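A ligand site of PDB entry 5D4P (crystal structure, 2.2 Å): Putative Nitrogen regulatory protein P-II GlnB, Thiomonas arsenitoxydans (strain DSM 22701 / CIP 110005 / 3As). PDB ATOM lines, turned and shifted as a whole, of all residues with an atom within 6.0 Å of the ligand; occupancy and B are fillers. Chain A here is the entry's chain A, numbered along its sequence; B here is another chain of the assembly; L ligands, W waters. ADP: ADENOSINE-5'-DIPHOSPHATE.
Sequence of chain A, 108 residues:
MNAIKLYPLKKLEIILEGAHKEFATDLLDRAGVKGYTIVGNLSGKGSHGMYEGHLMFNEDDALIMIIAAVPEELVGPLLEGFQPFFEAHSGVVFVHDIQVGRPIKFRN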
ATOM      1  N   ILE A  15      16.823 -22.946 -26.926  1.00  0.00           N
ATOM      2  CA  ILE A  15      15.903 -22.140 -26.121  1.00  0.00           C
ATOM      3  C   ILE A  15      15.997 -20.673 -26.525  1.00  0.00           C
ATOM      4  O   ILE A  15      17.067 -20.061 -26.455  1.00  0.00           O
ATOM      5  CB  ILE A  15      16.172 -22.267 -24.598  1.00  0.00           C
ATOM      6  CG1 ILE A  15      15.888 -23.690 -24.122  1.00  0.00           C
ATOM      7  CG2 ILE A  15      15.268 -21.315 -23.825  1.00  0.00           C
ATOM      8  CD1 ILE A  15      16.524 -24.035 -22.811  1.00  0.00           C
ATOM      9  N   LEU A  16      14.851 -20.121 -26.928  1.00  0.00           N
ATOM     10  CA  LEU A  16      14.807 -18.752 -27.407  1.00  0.00           C
ATOM     11  C   LEU A  16      13.379 -18.228 -27.326  1.00  0.00           C
ATOM     12  O   LEU A  16      12.454 -18.974 -27.003  1.00  0.00           O
ATOM     13  CB  LEU A  16      15.328 -18.640 -28.845  1.00  0.00           C
ATOM     14  CG  LEU A  16      14.862 -19.601 -29.933  1.00  0.00           C
ATOM     15  CD1 LEU A  16      13.403 -19.483 -30.187  1.00  0.00           C
ATOM     16  CD2 LEU A  16      15.604 -19.290 -31.217  1.00  0.00           C
ATOM     17  N   SER A  43       8.746 -20.768 -18.771  1.00  0.00           N
ATOM     18  CA  SER A  43       9.263 -19.578 -18.104  1.00  0.00           C
ATOM     19  C   SER A  43      10.772 -19.775 -17.931  1.00  0.00           C
ATOM     20  O   SER A  43      11.281 -20.855 -18.198  1.00  0.00           O
ATOM     21  CB  SER A  43       8.551 -19.324 -16.769  1.00  0.00           C
ATOM     22  OG  SER A  43       8.600 -20.454 -15.919  1.00  0.00           O
ATOM     23  N   GLY A  44      11.479 -18.755 -17.490  1.00  0.00           N
ATOM     24  CA  GLY A  44      12.893 -18.899 -17.253  1.00  0.00           C
ATOM     25  C   GLY A  44      13.559 -17.644 -16.739  1.00  0.00           C
ATOM     26  O   GLY A  44      13.001 -16.546 -16.798  1.00  0.00           O
ATOM     27  N   LYS A  45      14.787 -17.814 -16.263  1.00  0.00           N
ATOM     28  CA  LYS A  45      15.585 -16.685 -15.810  1.00  0.00           C
ATOM     29  C   LYS A  45      16.850 -16.605 -16.644  1.00  0.00           C
ATOM     30  O   LYS A  45      17.552 -17.597 -16.806  1.00  0.00           O
ATOM     31  CB  LYS A  45      15.949 -16.808 -14.337  1.00  0.00           C
ATOM     32  CG  LYS A  45      16.785 -15.633 -13.844  1.00  0.00           C
ATOM     33  CD  LYS A  45      17.334 -15.865 -12.444  1.00  0.00           C
ATOM     34  CE  LYS A  45      18.720 -16.494 -12.524  1.00  0.00           C
ATOM     35  NZ  LYS A  45      19.778 -15.528 -12.914  1.00  0.00           N
ATOM     36  N   GLY A  46      17.146 -15.420 -17.168  1.00  0.00           N
ATOM     37  CA  GLY A  46      18.370 -15.247 -17.914  1.00  0.00           C
ATOM     38  C   GLY A  46      19.304 -14.326 -17.165  1.00  0.00           C
ATOM     39  O   GLY A  46      19.038 -13.984 -16.011  1.00  0.00           O
ATOM     40  N   SER A  47      20.399 -13.950 -17.808  1.00  0.00           N
ATOM     41  CA  SER A  47      21.396 -13.075 -17.201  1.00  0.00           C
ATOM     42  C   SER A  47      20.848 -11.674 -16.854  1.00  0.00           C
ATOM     43  O   SER A  47      21.336 -11.024 -15.941  1.00  0.00           O
ATOM     44  CB  SER A  47      22.598 -12.932 -18.129  1.00  0.00           C
ATOM     45  OG  SER A  47      22.352 -11.985 -19.151  1.00  0.00           O
ATOM     46  N   HIS A  48      19.807 -11.246 -17.568  1.00  0.00           N
ATOM     47  CA  HIS A  48      19.324  -9.880 -17.454  1.00  0.00           C
ATOM     48  C   HIS A  48      17.853  -9.773 -17.039  1.00  0.00           C
ATOM     49  O   HIS A  48      17.463  -8.803 -16.404  1.00  0.00           O
ATOM     50  CB  HIS A  48      19.537  -9.126 -18.769  1.00  0.00           C
ATOM     51  N   GLY A  49      17.042 -10.759 -17.412  1.00  0.00           N
ATOM     52  CA  GLY A  49      15.625 -10.690 -17.111  1.00  0.00           C
ATOM     53  C   GLY A  49      14.927 -11.993 -16.754  1.00  0.00           C
ATOM     54  O   GLY A  49      15.518 -13.079 -16.820  1.00  0.00           O
ATOM     55  N   MET A  50      13.654 -11.869 -16.385  1.00  0.00           N
ATOM     56  CA  MET A  50      12.806 -13.017 -16.102  1.00  0.00           C
ATOM     57  C   MET A  50      11.876 -13.213 -17.298  1.00  0.00           C
ATOM     58  O   MET A  50      11.397 -12.247 -17.881  1.00  0.00           O
ATOM     59  CB  MET A  50      11.996 -12.800 -14.816  1.00  0.00           C
ATOM     60  CG  MET A  50      12.760 -13.024 -13.519  1.00  0.00           C
ATOM     61  SD  MET A  50      13.356 -14.720 -13.326  1.00  0.00           S
ATOM     62  CE  MET A  50      11.821 -15.660 -13.338  1.00  0.00           C
ATOM     63  N   TYR A  51      11.643 -14.459 -17.687  1.00  0.00           N
ATOM     64  CA  TYR A  51      10.643 -14.744 -18.710  1.00  0.00           C
ATOM     65  C   TYR A  51       9.469 -15.463 -18.086  1.00  0.00           C
ATOM     66  O   TYR A  51       9.566 -16.648 -17.751  1.00  0.00           O
ATOM     67  CB  TYR A  51      11.240 -15.568 -19.857  1.00  0.00           C
ATOM     68  CG  TYR A  51      12.249 -14.792 -20.658  1.00  0.00           C
ATOM     69  CD1 TYR A  51      13.549 -14.604 -20.182  1.00  0.00           C
ATOM     70  CD2 TYR A  51      11.910 -14.195 -21.877  1.00  0.00           C
ATOM     71  CE1 TYR A  51      14.476 -13.872 -20.894  1.00  0.00           C
ATOM     72  CE2 TYR A  51      12.839 -13.457 -22.602  1.00  0.00           C
ATOM     73  CZ  TYR A  51      14.124 -13.292 -22.100  1.00  0.00           C
ATOM     74  OH  TYR A  51      15.064 -12.562 -22.786  1.00  0.00           O
ATOM     75  N   LEU A  63       8.572 -17.688 -24.411  1.00  0.00           N
ATOM     76  CA  LEU A  63       9.807 -18.466 -24.498  1.00  0.00           C
ATOM     77  C   LEU A  63       9.526 -19.869 -25.045  1.00  0.00           C
ATOM     78  O   LEU A  63       8.560 -20.493 -24.610  1.00  0.00           O
ATOM     79  CB  LEU A  63      10.447 -18.521 -23.107  1.00  0.00           C
ATOM     80  CG  LEU A  63      11.911 -18.900 -22.941  1.00  0.00           C
ATOM     81  CD1 LEU A  63      12.742 -17.749 -23.471  1.00  0.00           C
ATOM     82  CD2 LEU A  63      12.207 -19.143 -21.481  1.00  0.00           C
ATOM     83  N   HIS A  89      20.707 -11.846 -29.626  1.00  0.00           N
ATOM     84  CA  HIS A  89      19.456 -12.180 -28.955  1.00  0.00           C
ATOM     85  C   HIS A  89      19.641 -13.140 -27.782  1.00  0.00           C
ATOM     86  O   HIS A  89      20.651 -13.843 -27.676  1.00  0.00           O
ATOM     87  CB  HIS A  89      18.467 -12.795 -29.953  1.00  0.00           C
ATOM     88  CG  HIS A  89      17.959 -11.826 -30.973  1.00  0.00           C
ATOM     89  ND1 HIS A  89      18.490 -11.743 -32.245  1.00  0.00           N
ATOM     90  CD2 HIS A  89      16.996 -10.876 -30.907  1.00  0.00           C
ATOM     91  CE1 HIS A  89      17.870 -10.787 -32.921  1.00  0.00           C
ATOM     92  NE2 HIS A  89      16.955 -10.247 -32.124  1.00  0.00           N
ATOM     93  N   SER A  90      18.625 -13.189 -26.918  1.00  0.00           N
ATOM     94  CA  SER A  90      18.635 -14.052 -25.742  1.00  0.00           C
ATOM     95  C   SER A  90      18.441 -15.535 -26.084  1.00  0.00           C
ATOM     96  O   SER A  90      17.855 -15.888 -27.115  1.00  0.00           O
ATOM     97  CB  SER A  90      17.536 -13.612 -24.769  1.00  0.00           C
ATOM     98  OG  SER A  90      17.820 -12.320 -24.271  1.00  0.00           O
ATOM     99  N   GLY A  91      18.950 -16.407 -25.216  1.00  0.00           N
ATOM    100  CA  GLY A  91      18.771 -17.855 -25.390  1.00  0.00           C
ATOM    101  C   GLY A  91      20.049 -18.661 -25.400  1.00  0.00           C
ATOM    102  O   GLY A  91      21.156 -18.103 -25.334  1.00  0.00           O
ATOM    103  N   VAL A  92      19.899 -19.985 -25.454  1.00  0.00           N
ATOM    104  CA  VAL A  92      21.024 -20.914 -25.392  1.00  0.00           C
ATOM    105  C   VAL A  92      20.779 -22.137 -26.251  1.00  0.00           C
ATOM    106  O   VAL A  92      19.628 -22.501 -26.527  1.00  0.00           O
ATOM    107  CB  VAL A  92      21.312 -21.402 -23.940  1.00  0.00           C
ATOM    108  CG1 VAL A  92      21.809 -20.240 -23.073  1.00  0.00           C
ATOM    109  CG2 VAL A  92      20.053 -22.080 -23.322  1.00  0.00           C
ATOM    110  N   PHE A  94      21.840 -26.237 -26.348  1.00  0.00           N
ATOM    111  CA  PHE A  94      22.486 -27.385 -25.709  1.00  0.00           C
ATOM    112  C   PHE A  94      22.707 -28.519 -26.745  1.00  0.00           C
ATOM    113  O   PHE A  94      21.789 -28.931 -27.450  1.00  0.00           O
ATOM    114  CB  PHE A  94      21.643 -27.927 -24.553  1.00  0.00           C
ATOM    115  CG  PHE A  94      21.291 -26.903 -23.498  1.00  0.00           C
ATOM    116  CD1 PHE A  94      22.183 -25.868 -23.172  1.00  0.00           C
ATOM    117  CD2 PHE A  94      20.072 -26.987 -22.836  1.00  0.00           C
ATOM    118  CE1 PHE A  94      21.862 -24.943 -22.195  1.00  0.00           C
ATOM    119  CE2 PHE A  94      19.742 -26.053 -21.832  1.00  0.00           C
ATOM    120  CZ  PHE A  94      20.640 -25.024 -21.524  1.00  0.00           C
ATOM    121  N   VAL B  33      24.251 -20.695 -10.308  1.00  0.00           N
ATOM    122  CA  VAL B  33      23.706 -21.043 -11.613  1.00  0.00           C
ATOM    123  C   VAL B  33      23.297 -19.756 -12.370  1.00  0.00           C
ATOM    124  O   VAL B  33      22.588 -18.909 -11.822  1.00  0.00           O
ATOM    125  CB  VAL B  33      22.508 -21.997 -11.444  1.00  0.00           C
ATOM    126  CG1 VAL B  33      21.827 -22.287 -12.765  1.00  0.00           C
ATOM    127  CG2 VAL B  33      22.940 -23.261 -10.743  1.00  0.00           C
ATOM    128  N   LYS B  34      23.757 -19.596 -13.601  1.00  0.00           N
ATOM    129  CA  LYS B  34      23.579 -18.307 -14.290  1.00  0.00           C
ATOM    130  C   LYS B  34      22.241 -18.193 -15.031  1.00  0.00           C
ATOM    131  O   LYS B  34      21.867 -17.116 -15.500  1.00  0.00           O
ATOM    132  CB  LYS B  34      24.743 -18.062 -15.263  1.00  0.00           C
ATOM    133  CG  LYS B  34      26.096 -17.912 -14.583  1.00  0.00           C
ATOM    134  N   GLY B  35      21.513 -19.291 -15.134  1.00  0.00           N
ATOM    135  CA  GLY B  35      20.191 -19.264 -15.755  1.00  0.00           C
ATOM    136  C   GLY B  35      19.459 -20.575 -15.580  1.00  0.00           C
ATOM    137  O   GLY B  35      20.083 -21.581 -15.214  1.00  0.00           O
ATOM    138  N   TYR B  36      18.156 -20.574 -15.836  1.00  0.00           N
ATOM    139  CA  TYR B  36      17.374 -21.808 -15.811  1.00  0.00           C
ATOM    140  C   TYR B  36      16.055 -21.635 -16.566  1.00  0.00           C
ATOM    141  O   TYR B  36      15.580 -20.507 -16.753  1.00  0.00           O
ATOM    142  CB  TYR B  36      17.099 -22.283 -14.355  1.00  0.00           C
ATOM    143  CG  TYR B  36      16.343 -21.307 -13.480  1.00  0.00           C
ATOM    144  CD1 TYR B  36      14.970 -21.165 -13.596  1.00  0.00           C
ATOM    145  CD2 TYR B  36      16.997 -20.538 -12.524  1.00  0.00           C
ATOM    146  CE1 TYR B  36      14.257 -20.281 -12.776  1.00  0.00           C
ATOM    147  CE2 TYR B  36      16.291 -19.640 -11.696  1.00  0.00           C
ATOM    148  CZ  TYR B  36      14.919 -19.520 -11.848  1.00  0.00           C
ATOM    149  OH  TYR B  36      14.195 -18.638 -11.064  1.00  0.00           O
ATOM    150  N   THR B  37      15.484 -22.761 -16.975  1.00  0.00           N
ATOM    151  CA  THR B  37      14.260 -22.825 -17.776  1.00  0.00           C
ATOM    152  C   THR B  37      13.241 -23.733 -17.087  1.00  0.00           C
ATOM    153  O   THR B  37      13.595 -24.800 -16.584  1.00  0.00           O
ATOM    154  CB  THR B  37      14.584 -23.333 -19.208  1.00  0.00           C
ATOM    155  OG1 THR B  37      15.563 -22.477 -19.771  1.00  0.00           O
ATOM    156  CG2 THR B  37      13.350 -23.345 -20.107  1.00  0.00           C
ATOM    157  N   ILE B  38      11.984 -23.313 -17.031  1.00  0.00           N
ATOM    158  CA  ILE B  38      10.989 -24.118 -16.347  1.00  0.00           C
ATOM    159  C   ILE B  38       9.925 -24.564 -17.314  1.00  0.00           C
ATOM    160  O   ILE B  38       9.362 -23.740 -18.039  1.00  0.00           O
ATOM    161  CB  ILE B  38      10.354 -23.344 -15.161  1.00  0.00           C
ATOM    162  CG1 ILE B  38      11.461 -22.872 -14.212  1.00  0.00           C
ATOM    163  CG2 ILE B  38       9.337 -24.204 -14.455  1.00  0.00           C
ATOM    164  CD1 ILE B  38      10.996 -22.128 -12.988  1.00  0.00           C
ATOM    165  N   ILE B  67      15.068 -26.956 -15.869  1.00  0.00           N
ATOM    166  CA  ILE B  67      16.255 -27.294 -16.663  1.00  0.00           C
ATOM    167  C   ILE B  67      17.350 -26.288 -16.388  1.00  0.00           C
ATOM    168  O   ILE B  67      17.161 -25.087 -16.580  1.00  0.00           O
ATOM    169  CB  ILE B  67      15.963 -27.271 -18.181  1.00  0.00           C
ATOM    170  CG1 ILE B  67      14.760 -28.151 -18.519  1.00  0.00           C
ATOM    171  CG2 ILE B  67      17.226 -27.660 -18.968  1.00  0.00           C
ATOM    172  CD1 ILE B  67      14.132 -27.824 -19.854  1.00  0.00           C
ATOM    173  N   ALA B  68      18.509 -26.772 -15.938  1.00  0.00           N
ATOM    174  CA  ALA B  68      19.590 -25.864 -15.579  1.00  0.00           C
ATOM    175  C   ALA B  68      20.927 -26.355 -16.103  1.00  0.00           C
ATOM    176  O   ALA B  68      21.395 -27.429 -15.717  1.00  0.00           O
ATOM    177  CB  ALA B  68      19.645 -25.657 -14.066  1.00  0.00           C
ATOM    178  N   ALA B  69      21.516 -25.590 -17.003  1.00  0.00           N
ATOM    179  CA  ALA B  69      22.850 -25.894 -17.503  1.00  0.00           C
ATOM    180  C   ALA B  69      23.901 -25.285 -16.583  1.00  0.00           C
ATOM    181  O   ALA B  69      23.887 -24.078 -16.343  1.00  0.00           O
ATOM    182  CB  ALA B  69      23.025 -25.411 -18.936  1.00  0.00           C
ATOM    183  N   VAL B  70      24.801 -26.114 -16.063  1.00  0.00           N
ATOM    184  CA  VAL B  70      25.761 -25.658 -15.065  1.00  0.00           C
ATOM    185  C   VAL B  70      27.136 -26.254 -15.269  1.00  0.00           C
ATOM    186  O   VAL B  70      27.255 -27.378 -15.736  1.00  0.00           O
ATOM    187  CB  VAL B  70      25.272 -25.993 -13.632  1.00  0.00           C
ATOM    188  CG1 VAL B  70      23.830 -25.549 -13.473  1.00  0.00           C
ATOM    189  CG2 VAL B  70      25.367 -27.499 -13.377  1.00  0.00           C
ATOM    190  N   LYS B 105      28.962 -17.803 -20.786  1.00  0.00           N
ATOM    191  CA  LYS B 105      27.551 -17.549 -20.566  1.00  0.00           C
ATOM    192  C   LYS B 105      27.019 -18.351 -19.363  1.00  0.00           C
ATOM    193  O   LYS B 105      25.983 -18.011 -18.787  1.00  0.00           O
ATOM    194  CB  LYS B 105      26.745 -17.885 -21.832  1.00  0.00           C
ATOM    195  CG  LYS B 105      25.266 -17.533 -21.698  1.00  0.00           C
ATOM    196  CD  LYS B 105      24.572 -17.415 -23.027  1.00  0.00           C
ATOM    197  CE  LYS B 105      23.129 -16.929 -22.839  1.00  0.00           C
ATOM    198  NZ  LYS B 105      23.060 -15.506 -22.391  1.00  0.00           N
ATOM    199  N   PHE B 106      27.744 -19.393 -18.977  1.00  0.00           N
ATOM    200  CA  PHE B 106      27.259 -20.306 -17.952  1.00  0.00           C
ATOM    201  C   PHE B 106      28.032 -20.218 -16.636  1.00  0.00           C
ATOM    202  O   PHE B 106      27.861 -21.065 -15.759  1.00  0.00           O
ATOM    203  CB  PHE B 106      27.260 -21.711 -18.503  1.00  0.00           C
ATOM    204  CG  PHE B 106      26.467 -21.836 -19.770  1.00  0.00           C
ATOM    205  CD1 PHE B 106      25.089 -22.029 -19.721  1.00  0.00           C
ATOM    206  CD2 PHE B 106      27.083 -21.675 -20.998  1.00  0.00           C
ATOM    207  CE1 PHE B 106      24.345 -22.117 -20.909  1.00  0.00           C
ATOM    208  CE2 PHE B 106      26.348 -21.762 -22.184  1.00  0.00           C
ATOM    209  CZ  PHE B 106      24.973 -21.987 -22.134  1.00  0.00           C
HETATM  210  PB  ADP L   1      18.906 -12.286 -20.928  1.00  0.00           P
HETATM  211  O1B ADP L   1      17.865 -12.117 -19.848  1.00  0.00           O
HETATM  212  O2B ADP L   1      18.691 -11.438 -22.149  1.00  0.00           O
HETATM  213  O3B ADP L   1      20.328 -12.259 -20.427  1.00  0.00           O
HETATM  214  PA  ADP L   1      19.622 -15.031 -21.577  1.00  0.00           P
HETATM  215  O1A ADP L   1      20.693 -14.955 -20.518  1.00  0.00           O
HETATM  216  O2A ADP L   1      20.007 -15.219 -23.031  1.00  0.00           O
HETATM  217  O3A ADP L   1      18.587 -13.788 -21.454  1.00  0.00           O
HETATM  218  O5' ADP L   1      18.667 -16.290 -21.245  1.00  0.00           O
HETATM  219  C5' ADP L   1      17.492 -16.487 -22.032  1.00  0.00           C
HETATM  220  C4' ADP L   1      16.705 -17.701 -21.566  1.00  0.00           C
HETATM  221  O4' ADP L   1      17.466 -18.871 -21.850  1.00  0.00           O
HETATM  222  C3' ADP L   1      16.471 -17.747 -20.055  1.00  0.00           C
HETATM  223  O3' ADP L   1      15.266 -17.106 -19.684  1.00  0.00           O
HETATM  224  C2' ADP L   1      16.422 -19.234 -19.773  1.00  0.00           C
HETATM  225  O2' ADP L   1      15.106 -19.713 -20.015  1.00  0.00           O
HETATM  226  C1' ADP L   1      17.335 -19.833 -20.814  1.00  0.00           C
HETATM  227  N9  ADP L   1      18.638 -20.023 -20.145  1.00  0.00           N
HETATM  228  C8  ADP L   1      19.636 -19.118 -20.018  1.00  0.00           C
HETATM  229  N7  ADP L   1      20.666 -19.633 -19.311  1.00  0.00           N
HETATM  230  C5  ADP L   1      20.310 -20.888 -18.967  1.00  0.00           C
HETATM  231  C6  ADP L   1      20.924 -22.009 -18.216  1.00  0.00           C
HETATM  232  N6  ADP L   1      22.169 -21.892 -17.666  1.00  0.00           N
HETATM  233  N1  ADP L   1      20.212 -23.148 -18.093  1.00  0.00           N
HETATM  234  C2  ADP L   1      18.976 -23.293 -18.630  1.00  0.00           C
HETATM  235  N3  ADP L   1      18.347 -22.328 -19.312  1.00  0.00           N
HETATM  236  C4  ADP L   1      18.971 -21.131 -19.514  1.00  0.00           C
HETATM  237  O   HOH W   1      23.379 -19.329 -18.290  1.00  0.00           O
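N of Ser 47 lies within hydrogen-bond range of O1A of the ligand (2.9 Å). O3B of the ligand sits at hydrogen-bond distance from OG of Ser 47 (2.4 Å). O2B of the ligand sits at hydrogen-bond distance from OG of Ser 90 (2.5 Å). The backbone NH (N) of Gly 91 lies within hydrogen-bond range of an oxygen (O2A) of the ligand, at 2.7 Å. The side-chain hydroxyl of Thr 37 of chain B lies within hydrogen-bond range of an oxygen (O2') of the ligand, 2.8 Å away. An oxygen (O1B) of the ligand sits at hydrogen-bond distance from the backbone NH (N) of Gly 49, at 2.9 Å. The backbone NH of Ala 69 of chain B sits at hydrogen-bond distance from a nitrogen (N1) of the ligand (3.0 Å). The backbone carbonyl oxygen (O) of Ala 69 of chain B sits at hydrogen-bond distance from a nitrogen (N6) of the ligand (3.1 Å). An oxygen (O1A) of the ligand is in salt-bridge range of the side-chain amino group of Lys 105 of chain B (3.1 Å). The backbone NH (N) of His 48 lies within hydrogen-bond range of an oxygen (O3B) of the ligand (3.1 Å). N6 of the ligand lies close to O of Gly 35 of chain B (3.2 Å). O of Tyr 36 of chain B lies close to O2' of the ligand (3.4 Å).
The side-chain hydroxyl of Ser 90 sits at hydrogen-bond distance from the side-chain hydroxyl of Tyr 51 (3.1 Å). O of Thr 37 of chain B lies within hydrogen-bond range of N of Ile 67 of chain B, at 2.7 Å. The backbone NH (N) of Tyr 51 is in hydrogen-bond range of the backbone carbonyl oxygen (O) of Gly 44 (2.6 Å). O of Tyr 36 of chain B lies within hydrogen-bond range of N of Lys 45 (2.8 Å). The backbone NH (N) of Ile 15 lies within hydrogen-bond range of the backbone carbonyl oxygen (O) of Val 92 (2.9 Å).
Merely in contact with the ligand: Ile 15, Gly 44, Lys 45, Gly 46, Tyr 51, Leu 63, Val 92, Phe 94, Ile 67 of chain B, Ala 68 of chain B and Phe 106 of chain B.
Water W1 lies within hydrogen-bond range of a nitrogen (N6) of the ligand (2.9 Å) and the backbone carbonyl oxygen (O) of Lys 105 of chain B (3.0 Å).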
